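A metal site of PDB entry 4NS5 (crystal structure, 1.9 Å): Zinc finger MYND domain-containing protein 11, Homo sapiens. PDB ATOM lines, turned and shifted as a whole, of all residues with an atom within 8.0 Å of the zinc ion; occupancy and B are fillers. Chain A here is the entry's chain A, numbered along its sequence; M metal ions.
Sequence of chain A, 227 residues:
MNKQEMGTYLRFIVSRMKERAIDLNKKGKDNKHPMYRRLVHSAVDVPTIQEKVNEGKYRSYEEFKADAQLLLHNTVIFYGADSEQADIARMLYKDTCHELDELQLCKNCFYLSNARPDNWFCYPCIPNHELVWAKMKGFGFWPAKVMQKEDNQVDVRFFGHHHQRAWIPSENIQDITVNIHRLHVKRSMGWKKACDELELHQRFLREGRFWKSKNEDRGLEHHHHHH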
ATOM      1  N   GLU A 102      -7.167   4.249  19.997  1.00  0.00           N
ATOM      2  CA  GLU A 102      -8.051   4.485  18.851  1.00  0.00           C
ATOM      3  C   GLU A 102      -7.245   4.749  17.593  1.00  0.00           C
ATOM      4  O   GLU A 102      -7.574   4.258  16.510  1.00  0.00           O
ATOM      5  CB  GLU A 102      -8.992   5.643  19.168  1.00  0.00           C
ATOM      6  CG  GLU A 102     -10.011   5.273  20.218  1.00  0.00           C
ATOM      7  CD  GLU A 102     -11.112   4.379  19.659  1.00  0.00           C
ATOM      8  OE1 GLU A 102     -11.758   4.794  18.679  1.00  0.00           O
ATOM      9  OE2 GLU A 102     -11.331   3.276  20.192  1.00  0.00           O
ATOM     10  N   LEU A 105      -6.094   1.481  16.320  1.00  0.00           N
ATOM     11  CA  LEU A 105      -7.194   0.741  15.712  1.00  0.00           C
ATOM     12  C   LEU A 105      -7.366   1.069  14.239  1.00  0.00           C
ATOM     13  O   LEU A 105      -7.502   0.161  13.417  1.00  0.00           O
ATOM     14  CB  LEU A 105      -8.528   1.041  16.415  1.00  0.00           C
ATOM     15  CG  LEU A 105      -9.023   0.086  17.502  1.00  0.00           C
ATOM     16  CD1 LEU A 105     -10.448   0.434  17.872  1.00  0.00           C
ATOM     17  CD2 LEU A 105      -8.922  -1.380  17.063  1.00  0.00           C
ATOM     18  N   CYS A 106      -7.395   2.353  13.899  1.00  0.00           N
ATOM     19  CA  CYS A 106      -7.446   2.792  12.511  1.00  0.00           C
ATOM     20  C   CYS A 106      -7.089   4.267  12.389  1.00  0.00           C
ATOM     21  O   CYS A 106      -7.827   5.132  12.805  1.00  0.00           O
ATOM     22  CB  CYS A 106      -8.823   2.541  11.902  1.00  0.00           C
ATOM     23  SG  CYS A 106      -8.993   3.161  10.204  1.00  0.00           S
ATOM     24  N   LYS A 107      -5.928   4.568  11.817  1.00  0.00           N
ATOM     25  CA  LYS A 107      -5.471   5.951  11.783  1.00  0.00           C
ATOM     26  C   LYS A 107      -6.358   6.811  10.909  1.00  0.00           C
ATOM     27  O   LYS A 107      -6.588   7.983  11.227  1.00  0.00           O
ATOM     28  CB  LYS A 107      -3.990   6.059  11.382  1.00  0.00           C
ATOM     29  CG  LYS A 107      -3.646   5.663   9.958  1.00  0.00           C
ATOM     30  CD  LYS A 107      -2.208   6.012   9.647  1.00  0.00           C
ATOM     31  CE  LYS A 107      -1.850   5.615   8.221  1.00  0.00           C
ATOM     32  NZ  LYS A 107      -0.497   6.101   7.836  1.00  0.00           N
ATOM     33  N   ASN A 108      -6.922   6.260   9.837  1.00  0.00           N
ATOM     34  CA  ASN A 108      -7.846   7.046   9.018  1.00  0.00           C
ATOM     35  C   ASN A 108      -9.102   7.484   9.770  1.00  0.00           C
ATOM     36  O   ASN A 108      -9.520   8.649   9.654  1.00  0.00           O
ATOM     37  CB  ASN A 108      -8.233   6.276   7.763  1.00  0.00           C
ATOM     38  CG  ASN A 108      -8.850   7.157   6.695  1.00  0.00           C
ATOM     39  OD1 ASN A 108      -9.866   6.785   6.081  1.00  0.00           O
ATOM     40  ND2 ASN A 108      -8.245   8.296   6.452  1.00  0.00           N
ATOM     41  N   CYS A 109      -9.709   6.559  10.498  1.00  0.00           N
ATOM     42  CA  CYS A 109     -10.848   6.864  11.363  1.00  0.00           C
ATOM     43  C   CYS A 109     -10.489   7.931  12.389  1.00  0.00           C
ATOM     44  O   CYS A 109     -11.239   8.852  12.632  1.00  0.00           O
ATOM     45  CB  CYS A 109     -11.335   5.616  12.118  1.00  0.00           C
ATOM     46  SG  CYS A 109     -12.362   4.508  11.105  1.00  0.00           S
ATOM     47  N   PHE A 110      -9.336   7.765  13.010  1.00  0.00           N
ATOM     48  CA  PHE A 110      -8.874   8.717  14.016  1.00  0.00           C
ATOM     49  C   PHE A 110      -8.700  10.092  13.379  1.00  0.00           C
ATOM     50  O   PHE A 110      -9.204  11.099  13.892  1.00  0.00           O
ATOM     51  CB  PHE A 110      -7.565   8.235  14.629  1.00  0.00           C
ATOM     52  CG  PHE A 110      -7.085   9.082  15.754  1.00  0.00           C
ATOM     53  CD1 PHE A 110      -6.178  10.105  15.540  1.00  0.00           C
ATOM     54  CD2 PHE A 110      -7.554   8.870  17.044  1.00  0.00           C
ATOM     55  CE1 PHE A 110      -5.736  10.895  16.607  1.00  0.00           C
ATOM     56  CE2 PHE A 110      -7.129   9.651  18.100  1.00  0.00           C
ATOM     57  CZ  PHE A 110      -6.218  10.671  17.873  1.00  0.00           C
ATOM     58  N   TYR A 111      -8.031  10.138  12.237  1.00  0.00           N
ATOM     59  CA  TYR A 111      -7.888  11.428  11.552  1.00  0.00           C
ATOM     60  C   TYR A 111      -9.236  12.078  11.272  1.00  0.00           C
ATOM     61  O   TYR A 111      -9.480  13.228  11.661  1.00  0.00           O
ATOM     62  CB  TYR A 111      -7.130  11.268  10.250  1.00  0.00           C
ATOM     63  CG  TYR A 111      -6.949  12.588   9.569  1.00  0.00           C
ATOM     64  CD1 TYR A 111      -5.925  13.442   9.953  1.00  0.00           C
ATOM     65  CD2 TYR A 111      -7.834  13.017   8.584  1.00  0.00           C
ATOM     66  CE1 TYR A 111      -5.769  14.671   9.350  1.00  0.00           C
ATOM     67  CE2 TYR A 111      -7.688  14.243   7.971  1.00  0.00           C
ATOM     68  CZ  TYR A 111      -6.643  15.069   8.362  1.00  0.00           C
ATOM     69  OH  TYR A 111      -6.491  16.284   7.777  1.00  0.00           O
ATOM     70  N   LEU A 112     -10.129  11.340  10.614  1.00  0.00           N
ATOM     71  CA  LEU A 112     -11.395  11.908  10.168  1.00  0.00           C
ATOM     72  C   LEU A 112     -12.326  12.283  11.303  1.00  0.00           C
ATOM     73  O   LEU A 112     -13.074  13.249  11.205  1.00  0.00           O
ATOM     74  CB  LEU A 112     -12.085  10.929   9.227  1.00  0.00           C
ATOM     75  CG  LEU A 112     -11.421  10.883   7.856  1.00  0.00           C
ATOM     76  CD1 LEU A 112     -11.917   9.701   7.040  1.00  0.00           C
ATOM     77  CD2 LEU A 112     -11.675  12.186   7.109  1.00  0.00           C
ATOM     78  N   PHE A 121     -17.459  10.501   8.141  1.00  0.00           N
ATOM     79  CA  PHE A 121     -17.655   9.070   8.457  1.00  0.00           C
ATOM     80  C   PHE A 121     -17.984   8.239   7.222  1.00  0.00           C
ATOM     81  O   PHE A 121     -18.078   7.002   7.310  1.00  0.00           O
ATOM     82  CB  PHE A 121     -18.761   8.947   9.488  1.00  0.00           C
ATOM     83  CG  PHE A 121     -18.806   7.610  10.202  1.00  0.00           C
ATOM     84  CD1 PHE A 121     -17.750   7.199  10.998  1.00  0.00           C
ATOM     85  CD2 PHE A 121     -19.958   6.827  10.141  1.00  0.00           C
ATOM     86  CE1 PHE A 121     -17.829   6.008  11.677  1.00  0.00           C
ATOM     87  CE2 PHE A 121     -20.033   5.629  10.838  1.00  0.00           C
ATOM     88  CZ  PHE A 121     -18.949   5.219  11.597  1.00  0.00           C
ATOM     89  N   TYR A 123     -16.124   8.443   4.253  1.00  0.00           N
ATOM     90  CA  TYR A 123     -14.964   8.130   3.490  1.00  0.00           C
ATOM     91  C   TYR A 123     -14.468   6.734   3.841  1.00  0.00           C
ATOM     92  O   TYR A 123     -14.487   6.318   5.001  1.00  0.00           O
ATOM     93  CB  TYR A 123     -13.899   9.186   3.694  1.00  0.00           C
ATOM     94  CG  TYR A 123     -14.299  10.449   3.057  1.00  0.00           C
ATOM     95  CD1 TYR A 123     -14.084  10.654   1.703  1.00  0.00           C
ATOM     96  CD2 TYR A 123     -14.935  11.449   3.799  1.00  0.00           C
ATOM     97  CE1 TYR A 123     -14.480  11.827   1.085  1.00  0.00           C
ATOM     98  CE2 TYR A 123     -15.335  12.625   3.194  1.00  0.00           C
ATOM     99  CZ  TYR A 123     -15.108  12.799   1.837  1.00  0.00           C
ATOM    100  OH  TYR A 123     -15.521  13.956   1.249  1.00  0.00           O
ATOM    101  N   PRO A 124     -14.046   5.982   2.832  1.00  0.00           N
ATOM    102  CA  PRO A 124     -13.550   4.633   3.070  1.00  0.00           C
ATOM    103  C   PRO A 124     -12.227   4.644   3.782  1.00  0.00           C
ATOM    104  O   PRO A 124     -11.514   5.664   3.744  1.00  0.00           O
ATOM    105  CB  PRO A 124     -13.339   4.064   1.660  1.00  0.00           C
ATOM    106  CG  PRO A 124     -13.805   5.080   0.701  1.00  0.00           C
ATOM    107  CD  PRO A 124     -13.977   6.369   1.412  1.00  0.00           C
ATOM    108  N   CYS A 125     -11.913   3.511   4.408  1.00  0.00           N
ATOM    109  CA  CYS A 125     -10.597   3.196   4.931  1.00  0.00           C
ATOM    110  C   CYS A 125     -10.025   1.980   4.206  1.00  0.00           C
ATOM    111  O   CYS A 125     -10.741   1.262   3.522  1.00  0.00           O
ATOM    112  CB  CYS A 125     -10.669   2.822   6.400  1.00  0.00           C
ATOM    113  SG  CYS A 125     -11.352   4.121   7.428  1.00  0.00           S
ATOM    114  N   ILE A 126      -8.723   1.745   4.403  1.00  0.00           N
ATOM    115  CA  ILE A 126      -8.052   0.554   3.885  1.00  0.00           C
ATOM    116  C   ILE A 126      -7.318  -0.192   5.016  1.00  0.00           C
ATOM    117  O   ILE A 126      -6.446   0.361   5.672  1.00  0.00           O
ATOM    118  CB  ILE A 126      -7.013   0.903   2.801  1.00  0.00           C
ATOM    119  CG1 ILE A 126      -7.637   1.765   1.705  1.00  0.00           C
ATOM    120  CG2 ILE A 126      -6.445  -0.370   2.174  1.00  0.00           C
ATOM    121  CD1 ILE A 126      -8.568   1.014   0.777  1.00  0.00           C
ATOM    122  N   PRO A 127      -7.704  -1.452   5.270  1.00  0.00           N
ATOM    123  CA  PRO A 127      -8.770  -2.164   4.611  1.00  0.00           C
ATOM    124  C   PRO A 127     -10.124  -1.563   4.988  1.00  0.00           C
ATOM    125  O   PRO A 127     -10.232  -0.781   5.927  1.00  0.00           O
ATOM    126  CB  PRO A 127      -8.644  -3.570   5.169  1.00  0.00           C
ATOM    127  CG  PRO A 127      -8.155  -3.360   6.549  1.00  0.00           C
ATOM    128  CD  PRO A 127      -7.248  -2.161   6.478  1.00  0.00           C
ATOM    129  N   ASN A 128     -11.132  -1.905   4.199  1.00  0.00           N
ATOM    130  CA  ASN A 128     -12.480  -1.454   4.419  1.00  0.00           C
ATOM    131  C   ASN A 128     -13.017  -2.022   5.716  1.00  0.00           C
ATOM    132  O   ASN A 128     -12.803  -3.193   5.999  1.00  0.00           O
ATOM    133  CB  ASN A 128     -13.391  -1.941   3.295  1.00  0.00           C
ATOM    134  CG  ASN A 128     -13.051  -1.341   1.949  1.00  0.00           C
ATOM    135  OD1 ASN A 128     -12.219  -0.443   1.799  1.00  0.00           O
ATOM    136  ND2 ASN A 128     -13.711  -1.841   0.947  1.00  0.00           N
ATOM    137  N   HIS A 129     -13.748  -1.233   6.493  1.00  0.00           N
ATOM    138  CA  HIS A 129     -14.447  -1.772   7.669  1.00  0.00           C
ATOM    139  C   HIS A 129     -15.593  -2.640   7.227  1.00  0.00           C
ATOM    140  O   HIS A 129     -16.306  -2.294   6.297  1.00  0.00           O
ATOM    141  CB  HIS A 129     -15.000  -0.652   8.550  1.00  0.00           C
ATOM    142  CG  HIS A 129     -13.925   0.166   9.183  1.00  0.00           C
ATOM    143  ND1 HIS A 129     -13.332  -0.192  10.369  1.00  0.00           N
ATOM    144  CD2 HIS A 129     -13.294   1.278   8.772  1.00  0.00           C
ATOM    145  CE1 HIS A 129     -12.402   0.679  10.679  1.00  0.00           C
ATOM    146  NE2 HIS A 129     -12.354   1.587   9.724  1.00  0.00           N
ATOM    147  N   LYS A 145     -20.029   0.436  11.654  1.00  0.00           N
ATOM    148  CA  LYS A 145     -18.742  -0.092  11.144  1.00  0.00           C
ATOM    149  C   LYS A 145     -18.082  -0.916  12.227  1.00  0.00           C
ATOM    150  O   LYS A 145     -18.040  -0.507  13.386  1.00  0.00           O
ATOM    151  CB  LYS A 145     -17.767   1.037  10.838  1.00  0.00           C
ATOM    152  CG  LYS A 145     -18.123   1.965   9.717  1.00  0.00           C
ATOM    153  CD  LYS A 145     -17.011   2.983   9.516  1.00  0.00           C
ATOM    154  CE  LYS A 145     -17.457   4.071   8.560  1.00  0.00           C
ATOM    155  NZ  LYS A 145     -16.388   5.059   8.269  1.00  0.00           N
ATOM    156  N   VAL A 146     -17.514  -2.060  11.856  1.00  0.00           N
ATOM    157  CA  VAL A 146     -16.828  -2.915  12.801  1.00  0.00           C
ATOM    158  C   VAL A 146     -15.414  -2.403  12.959  1.00  0.00           C
ATOM    159  O   VAL A 146     -14.703  -2.234  11.966  1.00  0.00           O
ATOM    160  CB  VAL A 146     -16.779  -4.373  12.320  1.00  0.00           C
ATOM    161  CG1 VAL A 146     -15.979  -5.214  13.283  1.00  0.00           C
ATOM    162  CG2 VAL A 146     -18.179  -4.920  12.169  1.00  0.00           C
ATOM    163  N   MET A 147     -15.003  -2.140  14.200  1.00  0.00           N
ATOM    164  CA  MET A 147     -13.646  -1.651  14.468  1.00  0.00           C
ATOM    165  C   MET A 147     -12.697  -2.797  14.818  1.00  0.00           C
ATOM    166  O   MET A 147     -11.532  -2.762  14.460  1.00  0.00           O
ATOM    167  CB  MET A 147     -13.649  -0.624  15.612  1.00  0.00           C
ATOM    168  CG  MET A 147     -14.481   0.619  15.365  1.00  0.00           C
ATOM    169  SD  MET A 147     -14.025   1.503  13.856  1.00  0.00           S
ATOM    170  CE  MET A 147     -12.410   2.158  14.291  1.00  0.00           C
HETATM  171 ZN    ZN M   1     -11.165   3.310   9.638  1.00  0.00          ZN
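The side-chain sulfur of Cys 125 lies close to the side-chain amide oxygen of Asn 108, 3.3 Å away.
The side-chain amide oxygen of Asn 128 lies close to the backbone carbonyl oxygen of Cys 125, 2.8 Å away.
O of Val 146 lies within hydrogen-bond range of ND1 of His 129.
N of Asn 108 sits close to SG of Cys 106 (3.7 Å).
The zinc ion is bound by NE2 of His 129, 2.1 Å away.
The zinc ion is bound by the side-chain sulfur (SG) of Cys 109, 2.2 Å away.
The zinc ion is bound by SG of Cys 106.
SG of Cys 125 is bound to the zinc ion, 2.4 Å away.
The zinc ion has four donor atoms within binding distance.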
